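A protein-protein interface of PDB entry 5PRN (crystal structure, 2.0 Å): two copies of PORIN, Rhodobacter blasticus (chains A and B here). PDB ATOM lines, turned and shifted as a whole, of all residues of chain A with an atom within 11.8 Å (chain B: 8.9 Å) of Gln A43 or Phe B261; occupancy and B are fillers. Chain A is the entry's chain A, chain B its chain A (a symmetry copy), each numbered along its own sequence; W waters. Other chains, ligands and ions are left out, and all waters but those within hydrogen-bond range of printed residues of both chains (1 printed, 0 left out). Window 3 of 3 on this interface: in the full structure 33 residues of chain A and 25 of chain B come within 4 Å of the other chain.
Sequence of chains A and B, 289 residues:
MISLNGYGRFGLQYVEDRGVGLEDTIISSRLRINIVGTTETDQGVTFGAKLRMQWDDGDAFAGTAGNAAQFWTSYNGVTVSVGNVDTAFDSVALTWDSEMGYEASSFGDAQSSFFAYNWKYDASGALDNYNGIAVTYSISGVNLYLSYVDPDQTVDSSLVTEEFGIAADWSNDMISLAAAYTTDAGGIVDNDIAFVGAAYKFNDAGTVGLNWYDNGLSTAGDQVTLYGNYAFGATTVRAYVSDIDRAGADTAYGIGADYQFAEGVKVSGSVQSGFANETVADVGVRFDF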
ATOM      1  N   THR A  39      -0.626  10.877  15.743  1.00  0.00           N
ATOM      2  CA  THR A  39       0.218  12.018  15.385  1.00  0.00           C
ATOM      3  C   THR A  39       0.314  11.967  13.840  1.00  0.00           C
ATOM      4  O   THR A  39       0.938  11.048  13.312  1.00  0.00           O
ATOM      5  CB  THR A  39       1.631  11.877  15.973  1.00  0.00           C
ATOM      6  OG1 THR A  39       1.510  11.756  17.435  1.00  0.00           O
ATOM      7  CG2 THR A  39       2.430  13.159  15.692  1.00  0.00           C
ATOM      8  N   GLU A  40      -0.311  12.923  13.176  1.00  0.00           N
ATOM      9  CA  GLU A  40      -0.275  12.954  11.698  1.00  0.00           C
ATOM     10  C   GLU A  40       0.807  13.923  11.244  1.00  0.00           C
ATOM     11  O   GLU A  40       1.073  14.958  11.878  1.00  0.00           O
ATOM     12  CB  GLU A  40      -1.628  13.541  11.191  1.00  0.00           C
ATOM     13  CG  GLU A  40      -2.938  12.597  11.557  1.00  0.00           C
ATOM     14  CD  GLU A  40      -4.181  13.253  11.155  1.00  0.00           C
ATOM     15  OE1 GLU A  40      -4.281  14.428  10.789  1.00  0.00           O
ATOM     16  OE2 GLU A  40      -5.205  12.550  11.365  1.00  0.00           O
ATOM     17  N   THR A  41       1.520  13.576  10.180  1.00  0.00           N
ATOM     18  CA  THR A  41       2.626  14.427   9.721  1.00  0.00           C
ATOM     19  C   THR A  41       2.329  14.915   8.287  1.00  0.00           C
ATOM     20  O   THR A  41       1.625  14.247   7.535  1.00  0.00           O
ATOM     21  CB  THR A  41       3.985  13.701   9.749  1.00  0.00           C
ATOM     22  OG1 THR A  41       3.999  12.614   8.826  1.00  0.00           O
ATOM     23  CG2 THR A  41       4.304  13.102  11.141  1.00  0.00           C
ATOM     24  N   ASP A  42       3.002  15.993   7.871  1.00  0.00           N
ATOM     25  CA  ASP A  42       2.853  16.454   6.491  1.00  0.00           C
ATOM     26  C   ASP A  42       3.602  15.574   5.514  1.00  0.00           C
ATOM     27  O   ASP A  42       3.398  15.746   4.308  1.00  0.00           O
ATOM     28  CB  ASP A  42       3.155  17.930   6.340  1.00  0.00           C
ATOM     29  CG  ASP A  42       4.526  18.380   6.750  1.00  0.00           C
ATOM     30  OD1 ASP A  42       5.453  17.581   6.952  1.00  0.00           O
ATOM     31  OD2 ASP A  42       4.741  19.592   6.903  1.00  0.00           O
ATOM     32  N   GLN A  43       4.425  14.622   5.958  1.00  0.00           N
ATOM     33  CA  GLN A  43       5.135  13.718   5.098  1.00  0.00           C
ATOM     34  C   GLN A  43       4.213  12.541   4.714  1.00  0.00           C
ATOM     35  O   GLN A  43       4.647  11.646   3.984  1.00  0.00           O
ATOM     36  CB  GLN A  43       6.416  13.176   5.744  1.00  0.00           C
ATOM     37  CG  GLN A  43       7.256  14.276   6.367  1.00  0.00           C
ATOM     38  CD  GLN A  43       7.764  15.230   5.307  1.00  0.00           C
ATOM     39  OE1 GLN A  43       8.287  14.772   4.295  1.00  0.00           O
ATOM     40  NE2 GLN A  43       7.631  16.529   5.468  1.00  0.00           N
ATOM     41  N   GLY A  44       3.018  12.468   5.277  1.00  0.00           N
ATOM     42  CA  GLY A  44       2.105  11.368   4.958  1.00  0.00           C
ATOM     43  C   GLY A  44       2.291  10.135   5.832  1.00  0.00           C
ATOM     44  O   GLY A  44       1.748   9.061   5.505  1.00  0.00           O
ATOM     45  N   VAL A  45       3.063  10.205   6.905  1.00  0.00           N
ATOM     46  CA  VAL A  45       3.277   9.102   7.817  1.00  0.00           C
ATOM     47  C   VAL A  45       2.446   9.352   9.083  1.00  0.00           C
ATOM     48  O   VAL A  45       2.582  10.433   9.651  1.00  0.00           O
ATOM     49  CB  VAL A  45       4.759   8.987   8.239  1.00  0.00           C
ATOM     50  CG1 VAL A  45       5.008   7.800   9.140  1.00  0.00           C
ATOM     51  CG2 VAL A  45       5.627   8.915   6.961  1.00  0.00           C
ATOM     52  N   THR A  46       1.616   8.395   9.463  1.00  0.00           N
ATOM     53  CA  THR A  46       0.844   8.606  10.713  1.00  0.00           C
ATOM     54  C   THR A  46       1.444   7.739  11.806  1.00  0.00           C
ATOM     55  O   THR A  46       1.850   6.616  11.487  1.00  0.00           O
ATOM     56  CB  THR A  46      -0.608   8.150  10.475  1.00  0.00           C
ATOM     57  OG1 THR A  46      -1.137   9.056   9.509  1.00  0.00           O
ATOM     58  CG2 THR A  46      -1.468   8.298  11.745  1.00  0.00           C
ATOM     59  N   PHE A  47       1.484   8.235  13.019  1.00  0.00           N
ATOM     60  CA  PHE A  47       1.954   7.419  14.166  1.00  0.00           C
ATOM     61  C   PHE A  47       0.744   7.328  15.115  1.00  0.00           C
ATOM     62  O   PHE A  47       0.000   8.312  15.261  1.00  0.00           O
ATOM     63  CB  PHE A  47       3.140   7.976  14.917  1.00  0.00           C
ATOM     64  CG  PHE A  47       4.395   8.053  14.068  1.00  0.00           C
ATOM     65  CD1 PHE A  47       4.538   9.108  13.161  1.00  0.00           C
ATOM     66  CD2 PHE A  47       5.392   7.093  14.186  1.00  0.00           C
ATOM     67  CE1 PHE A  47       5.690   9.186  12.389  1.00  0.00           C
ATOM     68  CE2 PHE A  47       6.533   7.186  13.425  1.00  0.00           C
ATOM     69  CZ  PHE A  47       6.682   8.240  12.509  1.00  0.00           C
ATOM     70  N   GLY A  48       0.534   6.142  15.695  1.00  0.00           N
ATOM     71  CA  GLY A  48      -0.581   5.998  16.612  1.00  0.00           C
ATOM     72  C   GLY A  48      -0.246   5.044  17.753  1.00  0.00           C
ATOM     73  O   GLY A  48       0.662   4.209  17.654  1.00  0.00           O
ATOM     74  N   TRP A  72       1.656   1.954  16.254  1.00  0.00           N
ATOM     75  CA  TRP A  72       1.694   1.707  14.814  1.00  0.00           C
ATOM     76  C   TRP A  72       2.219   2.924  14.068  1.00  0.00           C
ATOM     77  O   TRP A  72       2.170   4.052  14.537  1.00  0.00           O
ATOM     78  CB  TRP A  72       0.388   1.232  14.213  1.00  0.00           C
ATOM     79  CG  TRP A  72      -0.648   2.302  14.097  1.00  0.00           C
ATOM     80  CD1 TRP A  72      -0.840   3.188  13.049  1.00  0.00           C
ATOM     81  CD2 TRP A  72      -1.645   2.613  15.072  1.00  0.00           C
ATOM     82  NE1 TRP A  72      -1.892   4.016  13.345  1.00  0.00           N
ATOM     83  CE2 TRP A  72      -2.400   3.675  14.575  1.00  0.00           C
ATOM     84  CE3 TRP A  72      -1.947   2.058  16.334  1.00  0.00           C
ATOM     85  CZ2 TRP A  72      -3.470   4.232  15.282  1.00  0.00           C
ATOM     86  CZ3 TRP A  72      -3.000   2.611  17.031  1.00  0.00           C
ATOM     87  CH2 TRP A  72      -3.739   3.682  16.498  1.00  0.00           C
ATOM     88  N   THR A  73       2.703   2.615  12.854  1.00  0.00           N
ATOM     89  CA  THR A  73       3.175   3.576  11.900  1.00  0.00           C
ATOM     90  C   THR A  73       2.547   3.187  10.535  1.00  0.00           C
ATOM     91  O   THR A  73       2.675   2.006  10.155  1.00  0.00           O
ATOM     92  CB  THR A  73       4.712   3.519  11.691  1.00  0.00           C
ATOM     93  OG1 THR A  73       5.351   3.623  12.985  1.00  0.00           O
ATOM     94  CG2 THR A  73       5.114   4.797  10.943  1.00  0.00           C
ATOM     95  N   SER A  74       1.902   4.127   9.881  1.00  0.00           N
ATOM     96  CA  SER A  74       1.248   3.917   8.610  1.00  0.00           C
ATOM     97  C   SER A  74       1.756   4.853   7.503  1.00  0.00           C
ATOM     98  O   SER A  74       1.920   6.044   7.760  1.00  0.00           O
ATOM     99  CB  SER A  74      -0.275   4.177   8.686  1.00  0.00           C
ATOM    100  OG  SER A  74      -0.884   3.274   7.779  1.00  0.00           O
ATOM    101  N   TYR A  75       1.942   4.272   6.316  1.00  0.00           N
ATOM    102  CA  TYR A  75       2.393   5.081   5.179  1.00  0.00           C
ATOM    103  C   TYR A  75       2.023   4.349   3.884  1.00  0.00           C
ATOM    104  O   TYR A  75       2.382   3.200   3.717  1.00  0.00           O
ATOM    105  CB  TYR A  75       3.897   5.287   5.215  1.00  0.00           C
ATOM    106  CG  TYR A  75       4.454   6.048   4.034  1.00  0.00           C
ATOM    107  CD1 TYR A  75       4.104   7.380   3.824  1.00  0.00           C
ATOM    108  CD2 TYR A  75       5.323   5.440   3.143  1.00  0.00           C
ATOM    109  CE1 TYR A  75       4.608   8.072   2.756  1.00  0.00           C
ATOM    110  CE2 TYR A  75       5.849   6.131   2.050  1.00  0.00           C
ATOM    111  CZ  TYR A  75       5.472   7.447   1.879  1.00  0.00           C
ATOM    112  OH  TYR A  75       5.964   8.169   0.814  1.00  0.00           O
ATOM    113  N   ASN A  76       1.281   5.050   3.036  1.00  0.00           N
ATOM    114  CA  ASN A  76       0.929   4.530   1.727  1.00  0.00           C
ATOM    115  C   ASN A  76       0.268   3.170   1.746  1.00  0.00           C
ATOM    116  O   ASN A  76       0.761   2.284   1.007  1.00  0.00           O
ATOM    117  CB  ASN A  76       2.259   4.364   0.937  1.00  0.00           C
ATOM    118  CG  ASN A  76       2.417   5.472  -0.093  1.00  0.00           C
ATOM    119  OD1 ASN A  76       2.451   6.647   0.277  1.00  0.00           O
ATOM    120  ND2 ASN A  76       2.496   5.165  -1.370  1.00  0.00           N
ATOM    121  N   GLY A  77      -0.748   2.964   2.569  1.00  0.00           N
ATOM    122  CA  GLY A  77      -1.423   1.676   2.598  1.00  0.00           C
ATOM    123  C   GLY A  77      -0.720   0.640   3.474  1.00  0.00           C
ATOM    124  O   GLY A  77      -1.255  -0.461   3.660  1.00  0.00           O
ATOM    125  N   VAL A  78       0.520   0.831   3.864  1.00  0.00           N
ATOM    126  CA  VAL A  78       1.227  -0.162   4.666  1.00  0.00           C
ATOM    127  C   VAL A  78       1.142   0.249   6.154  1.00  0.00           C
ATOM    128  O   VAL A  78       1.387   1.422   6.440  1.00  0.00           O
ATOM    129  CB  VAL A  78       2.722  -0.243   4.297  1.00  0.00           C
ATOM    130  CG1 VAL A  78       3.418  -1.303   5.137  1.00  0.00           C
ATOM    131  CG2 VAL A  78       2.880  -0.578   2.814  1.00  0.00           C
ATOM    132  N   ALA B 234      17.632  19.913  10.980  1.00  0.00           N
ATOM    133  CA  ALA B 234      16.715  19.107  11.781  1.00  0.00           C
ATOM    134  C   ALA B 234      17.434  18.083  12.660  1.00  0.00           C
ATOM    135  O   ALA B 234      16.814  17.413  13.500  1.00  0.00           O
ATOM    136  CB  ALA B 234      15.728  18.375  10.866  1.00  0.00           C
ATOM    137  N   THR B 235      18.741  17.955  12.479  1.00  0.00           N
ATOM    138  CA  THR B 235      19.530  16.997  13.250  1.00  0.00           C
ATOM    139  C   THR B 235      20.278  17.609  14.400  1.00  0.00           C
ATOM    140  O   THR B 235      20.931  18.658  14.197  1.00  0.00           O
ATOM    141  CB  THR B 235      20.554  16.360  12.291  1.00  0.00           C
ATOM    142  OG1 THR B 235      19.839  15.767  11.218  1.00  0.00           O
ATOM    143  CG2 THR B 235      21.394  15.317  13.036  1.00  0.00           C
ATOM    144  N   ASP B 258      19.578  13.274  17.503  1.00  0.00           N
ATOM    145  CA  ASP B 258      18.154  13.396  17.343  1.00  0.00           C
ATOM    146  C   ASP B 258      17.848  13.954  15.925  1.00  0.00           C
ATOM    147  O   ASP B 258      18.560  14.859  15.419  1.00  0.00           O
ATOM    148  CB  ASP B 258      17.465  14.293  18.327  1.00  0.00           C
ATOM    149  CG  ASP B 258      17.794  14.069  19.797  1.00  0.00           C
ATOM    150  OD1 ASP B 258      17.762  12.887  20.291  1.00  0.00           O
ATOM    151  OD2 ASP B 258      18.076  15.085  20.543  1.00  0.00           O
ATOM    152  N   TYR B 259      16.769  13.439  15.378  1.00  0.00           N
ATOM    153  CA  TYR B 259      16.307  13.937  14.074  1.00  0.00           C
ATOM    154  C   TYR B 259      14.821  14.293  14.188  1.00  0.00           C
ATOM    155  O   TYR B 259      13.977  13.451  14.534  1.00  0.00           O
ATOM    156  CB  TYR B 259      16.597  12.945  12.983  1.00  0.00           C
ATOM    157  CG  TYR B 259      16.039  13.356  11.626  1.00  0.00           C
ATOM    158  CD1 TYR B 259      16.744  14.311  10.894  1.00  0.00           C
ATOM    159  CD2 TYR B 259      14.889  12.822  11.079  1.00  0.00           C
ATOM    160  CE1 TYR B 259      16.297  14.737   9.651  1.00  0.00           C
ATOM    161  CE2 TYR B 259      14.427  13.237   9.824  1.00  0.00           C
ATOM    162  CZ  TYR B 259      15.145  14.190   9.134  1.00  0.00           C
ATOM    163  OH  TYR B 259      14.721  14.623   7.883  1.00  0.00           O
ATOM    164  N   GLN B 260      14.552  15.564  13.965  1.00  0.00           N
ATOM    165  CA  GLN B 260      13.174  16.106  14.042  1.00  0.00           C
ATOM    166  C   GLN B 260      12.479  15.855  12.711  1.00  0.00           C
ATOM    167  O   GLN B 260      12.536  16.625  11.731  1.00  0.00           O
ATOM    168  CB  GLN B 260      13.224  17.555  14.448  1.00  0.00           C
ATOM    169  CG  GLN B 260      11.894  18.159  14.916  1.00  0.00           C
ATOM    170  CD  GLN B 260      11.508  17.697  16.317  1.00  0.00           C
ATOM    171  OE1 GLN B 260      12.340  17.701  17.246  1.00  0.00           O
ATOM    172  NE2 GLN B 260      10.256  17.305  16.577  1.00  0.00           N
ATOM    173  N   PHE B 261      11.847  14.716  12.617  1.00  0.00           N
ATOM    174  CA  PHE B 261      11.142  14.242  11.456  1.00  0.00           C
ATOM    175  C   PHE B 261       9.959  15.167  11.094  1.00  0.00           C
ATOM    176  O   PHE B 261       9.698  15.334   9.895  1.00  0.00           O
ATOM    177  CB  PHE B 261      10.647  12.811  11.690  1.00  0.00           C
ATOM    178  CG  PHE B 261       9.897  12.208  10.537  1.00  0.00           C
ATOM    179  CD1 PHE B 261      10.563  11.747   9.406  1.00  0.00           C
ATOM    180  CD2 PHE B 261       8.524  12.085  10.570  1.00  0.00           C
ATOM    181  CE1 PHE B 261       9.878  11.198   8.339  1.00  0.00           C
ATOM    182  CE2 PHE B 261       7.827  11.531   9.517  1.00  0.00           C
ATOM    183  CZ  PHE B 261       8.492  11.078   8.394  1.00  0.00           C
ATOM    184  N   ALA B 262       9.260  15.654  12.083  1.00  0.00           N
ATOM    185  CA  ALA B 262       8.080  16.496  11.872  1.00  0.00           C
ATOM    186  C   ALA B 262       7.730  17.085  13.228  1.00  0.00           C
ATOM    187  O   ALA B 262       8.382  16.684  14.215  1.00  0.00           O
ATOM    188  CB  ALA B 262       6.907  15.682  11.335  1.00  0.00           C
ATOM    189  N   GLU B 263       6.797  18.004  13.299  1.00  0.00           N
ATOM    190  CA  GLU B 263       6.371  18.556  14.567  1.00  0.00           C
ATOM    191  C   GLU B 263       5.814  17.385  15.433  1.00  0.00           C
ATOM    192  O   GLU B 263       4.983  16.618  14.899  1.00  0.00           O
ATOM    193  CB  GLU B 263       5.245  19.562  14.293  1.00  0.00           C
ATOM    194  CG  GLU B 263       4.890  20.411  15.503  1.00  0.00           C
ATOM    195  CD  GLU B 263       3.804  21.450  15.195  1.00  0.00           C
ATOM    196  OE1 GLU B 263       3.707  21.961  14.052  1.00  0.00           O
ATOM    197  OE2 GLU B 263       3.019  21.741  16.142  1.00  0.00           O
ATOM    198  N   GLY B 264       6.275  17.206  16.647  1.00  0.00           N
ATOM    199  CA  GLY B 264       5.736  16.082  17.428  1.00  0.00           C
ATOM    200  C   GLY B 264       6.389  14.742  17.161  1.00  0.00           C
ATOM    201  O   GLY B 264       5.949  13.757  17.811  1.00  0.00           O
ATOM    202  N   VAL B 265       7.316  14.557  16.225  1.00  0.00           N
ATOM    203  CA  VAL B 265       7.890  13.246  15.942  1.00  0.00           C
ATOM    204  C   VAL B 265       9.437  13.353  15.915  1.00  0.00           C
ATOM    205  O   VAL B 265      10.011  14.058  15.058  1.00  0.00           O
ATOM    206  CB  VAL B 265       7.458  12.635  14.608  1.00  0.00           C
ATOM    207  CG1 VAL B 265       8.058  11.244  14.385  1.00  0.00           C
ATOM    208  CG2 VAL B 265       5.920  12.592  14.453  1.00  0.00           C
ATOM    209  N   LYS B 266      10.078  12.627  16.822  1.00  0.00           N
ATOM    210  CA  LYS B 266      11.550  12.775  16.939  1.00  0.00           C
ATOM    211  C   LYS B 266      12.184  11.397  16.885  1.00  0.00           C
ATOM    212  O   LYS B 266      11.736  10.508  17.656  1.00  0.00           O
ATOM    213  CB  LYS B 266      11.832  13.494  18.255  1.00  0.00           C
ATOM    214  CG  LYS B 266      13.308  13.689  18.566  1.00  0.00           C
ATOM    215  CD  LYS B 266      13.526  14.734  19.613  1.00  0.00           C
ATOM    216  CE  LYS B 266      13.623  14.189  21.022  1.00  0.00           C
ATOM    217  NZ  LYS B 266      13.434  15.394  21.947  1.00  0.00           N
ATOM    218  N   VAL B 267      13.164  11.190  16.009  1.00  0.00           N
ATOM    219  CA  VAL B 267      13.843   9.885  15.924  1.00  0.00           C
ATOM    220  C   VAL B 267      15.187  10.002  16.636  1.00  0.00           C
ATOM    221  O   VAL B 267      15.864  11.031  16.420  1.00  0.00           O
ATOM    222  CB  VAL B 267      14.106   9.532  14.452  1.00  0.00           C
ATOM    223  CG1 VAL B 267      14.792   8.157  14.281  1.00  0.00           C
ATOM    224  CG2 VAL B 267      12.756   9.508  13.737  1.00  0.00           C
ATOM    225  N   SER B 268      15.506   9.185  17.636  1.00  0.00           N
ATOM    226  CA  SER B 268      16.756   9.411  18.345  1.00  0.00           C
ATOM    227  C   SER B 268      17.478   8.089  18.565  1.00  0.00           C
ATOM    228  O   SER B 268      16.858   7.018  18.558  1.00  0.00           O
ATOM    229  CB  SER B 268      16.614   9.980  19.761  1.00  0.00           C
ATOM    230  OG  SER B 268      15.669  11.040  19.767  1.00  0.00           O
ATOM    231  N   GLY B 284      15.224   4.666  18.314  1.00  0.00           N
ATOM    232  CA  GLY B 284      13.767   4.607  18.296  1.00  0.00           C
ATOM    233  C   GLY B 284      13.114   5.939  17.972  1.00  0.00           C
ATOM    234  O   GLY B 284      13.732   6.933  17.554  1.00  0.00           O
ATOM    235  N   VAL B 285      11.806   5.967  18.160  1.00  0.00           N
ATOM    236  CA  VAL B 285      11.014   7.141  17.794  1.00  0.00           C
ATOM    237  C   VAL B 285      10.034   7.462  18.918  1.00  0.00           C
ATOM    238  O   VAL B 285       9.472   6.564  19.543  1.00  0.00           O
ATOM    239  CB  VAL B 285      10.274   6.954  16.448  1.00  0.00           C
ATOM    240  CG1 VAL B 285       9.382   5.743  16.480  1.00  0.00           C
ATOM    241  CG2 VAL B 285       9.481   8.194  16.048  1.00  0.00           C
ATOM    242  N   ARG B 286       9.865   8.772  19.081  1.00  0.00           N
ATOM    243  CA  ARG B 286       8.868   9.284  19.996  1.00  0.00           C
ATOM    244  C   ARG B 286       7.869  10.162  19.214  1.00  0.00           C
ATOM    245  O   ARG B 286       8.297  11.055  18.431  1.00  0.00           O
ATOM    246  CB  ARG B 286       9.502  10.115  21.143  1.00  0.00           C
ATOM    247  CG  ARG B 286       8.422  10.887  21.963  1.00  0.00           C
ATOM    248  CD  ARG B 286       9.038  11.638  23.139  1.00  0.00           C
ATOM    249  NE  ARG B 286       8.078  12.682  23.602  1.00  0.00           N
ATOM    250  CZ  ARG B 286       8.088  13.163  24.844  1.00  0.00           C
ATOM    251  NH1 ARG B 286       9.024  12.689  25.680  1.00  0.00           N
ATOM    252  NH2 ARG B 286       7.233  14.089  25.241  1.00  0.00           N
ATOM    253  N   PHE B 287       6.591  10.042  19.472  1.00  0.00           N
ATOM    254  CA  PHE B 287       5.566  10.859  18.864  1.00  0.00           C
ATOM    255  C   PHE B 287       4.597  11.364  19.928  1.00  0.00           C
ATOM    256  O   PHE B 287       4.136  10.628  20.804  1.00  0.00           O
ATOM    257  CB  PHE B 287       4.898  10.138  17.682  1.00  0.00           C
ATOM    258  CG  PHE B 287       4.310   8.784  18.061  1.00  0.00           C
ATOM    259  CD1 PHE B 287       5.065   7.651  18.081  1.00  0.00           C
ATOM    260  CD2 PHE B 287       2.963   8.733  18.422  1.00  0.00           C
ATOM    261  CE1 PHE B 287       4.504   6.411  18.404  1.00  0.00           C
ATOM    262  CE2 PHE B 287       2.395   7.501  18.728  1.00  0.00           C
ATOM    263  CZ  PHE B 287       3.173   6.356  18.737  1.00  0.00           C
HETATM  264  O   HOH W   1       3.340  16.543  12.944  1.00  0.00           O
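O of Gly A48 sits at hydrogen-bond distance from N of Trp A72, at 2.8 Å.
The side-chain carboxylate of Asp A42 sits at hydrogen-bond distance from the side-chain amide nitrogen of Gln A43 (2.8 Å).
OG1 of Thr A41 sits at hydrogen-bond distance from O of Val A45, at 2.7 Å.
The backbone NH of Thr A39 lies within hydrogen-bond range of the backbone carbonyl oxygen of Phe A47.
The side-chain amide nitrogen (NE2) of Gln B260 lies within hydrogen-bond range of the backbone carbonyl oxygen (O) of Ala B262.
Among the printed residues, pairs that only touch across the chains: Phe A47 with Phe B287 (3.5 Å), Gly A48 with Phe B287 (3.5 Å), Thr A39 with Phe B287 (3.5 Å), Thr A41 with Ala B262 (3.7 Å), Phe A47 with Val B265 (3.7 Å), Thr A41 with Val B265 (3.7 Å), Thr A39 with Val B265 (3.7 Å), Val A45 with Phe B261 (3.9 Å) and Gln A43 with Phe B261 (3.97 Å).
Printed residues of chain A within 4 Å of Phe B261: Gln A43 (3.97 Å) and Val A45 (3.9 Å).
No residue of chain B comes within 4 Å of Asp A42.
No residue of chain B comes within 4 Å of Gly A44.
Tyr B259 touches none of the printed residues of chain A.
No residue of chain A comes within 4 Å of Gln B260.
Of chain A, only Thr A41 comes within 4 Å of Ala B262.
Val B265 touches just these residues of chain A: Thr A39, Thr A41 and Phe A47.
Val B267 touches none of the printed residues of chain A.
Printed residues of chain A within 4 Å of Phe B287: Thr A39 (3.5 Å), Phe A47 (3.5 Å) and Gly A48 (3.5 Å).
Of the printed residues of chain B, Thr A41 touches Ala B262 and Val B265.
Of the printed residues of chain B, Val A45 touches Phe B261.
Printed residues of chain B within 4 Å of Thr A39: Val B265 (3.7 Å) and Phe B287 (3.5 Å).
Arg B286 touches none of the printed residues of chain A.
The nearest residue of chain B that does not touch Gln A43 is Ala B262 (5.2 Å).
The nearest printed residue of chain B that does not touch Val A45 is Val B265 (6.2 Å).
Of the 17 printed residues of chain B, 4 touch a printed residue of chain A.
Printed residues of chain B that touch a printed residue of chain A: Phe B261, Ala B262, Val B265 and Phe B287.
Along chain B the printed residues that touch a printed residue of chain A span positions 261 to 287.
Of the 17 printed residues of chain A, 6 touch a printed residue of chain B.
Hydrophobic or aromatic side chains of chain A within 4 Å of the printed part of chain B: Val A45 and Phe A47.
Among the printed residues, no Asp or Glu carboxylate lies within 4 Å of a Lys or Arg side-chain nitrogen of the other chain.
No position is printed for both chains.
Of the 9 pairs that touch across the chains among the printed residues, none has its exchanged pair printed and touching as well.
Water W1 bridges O of Glu B263 and O of Glu A40.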
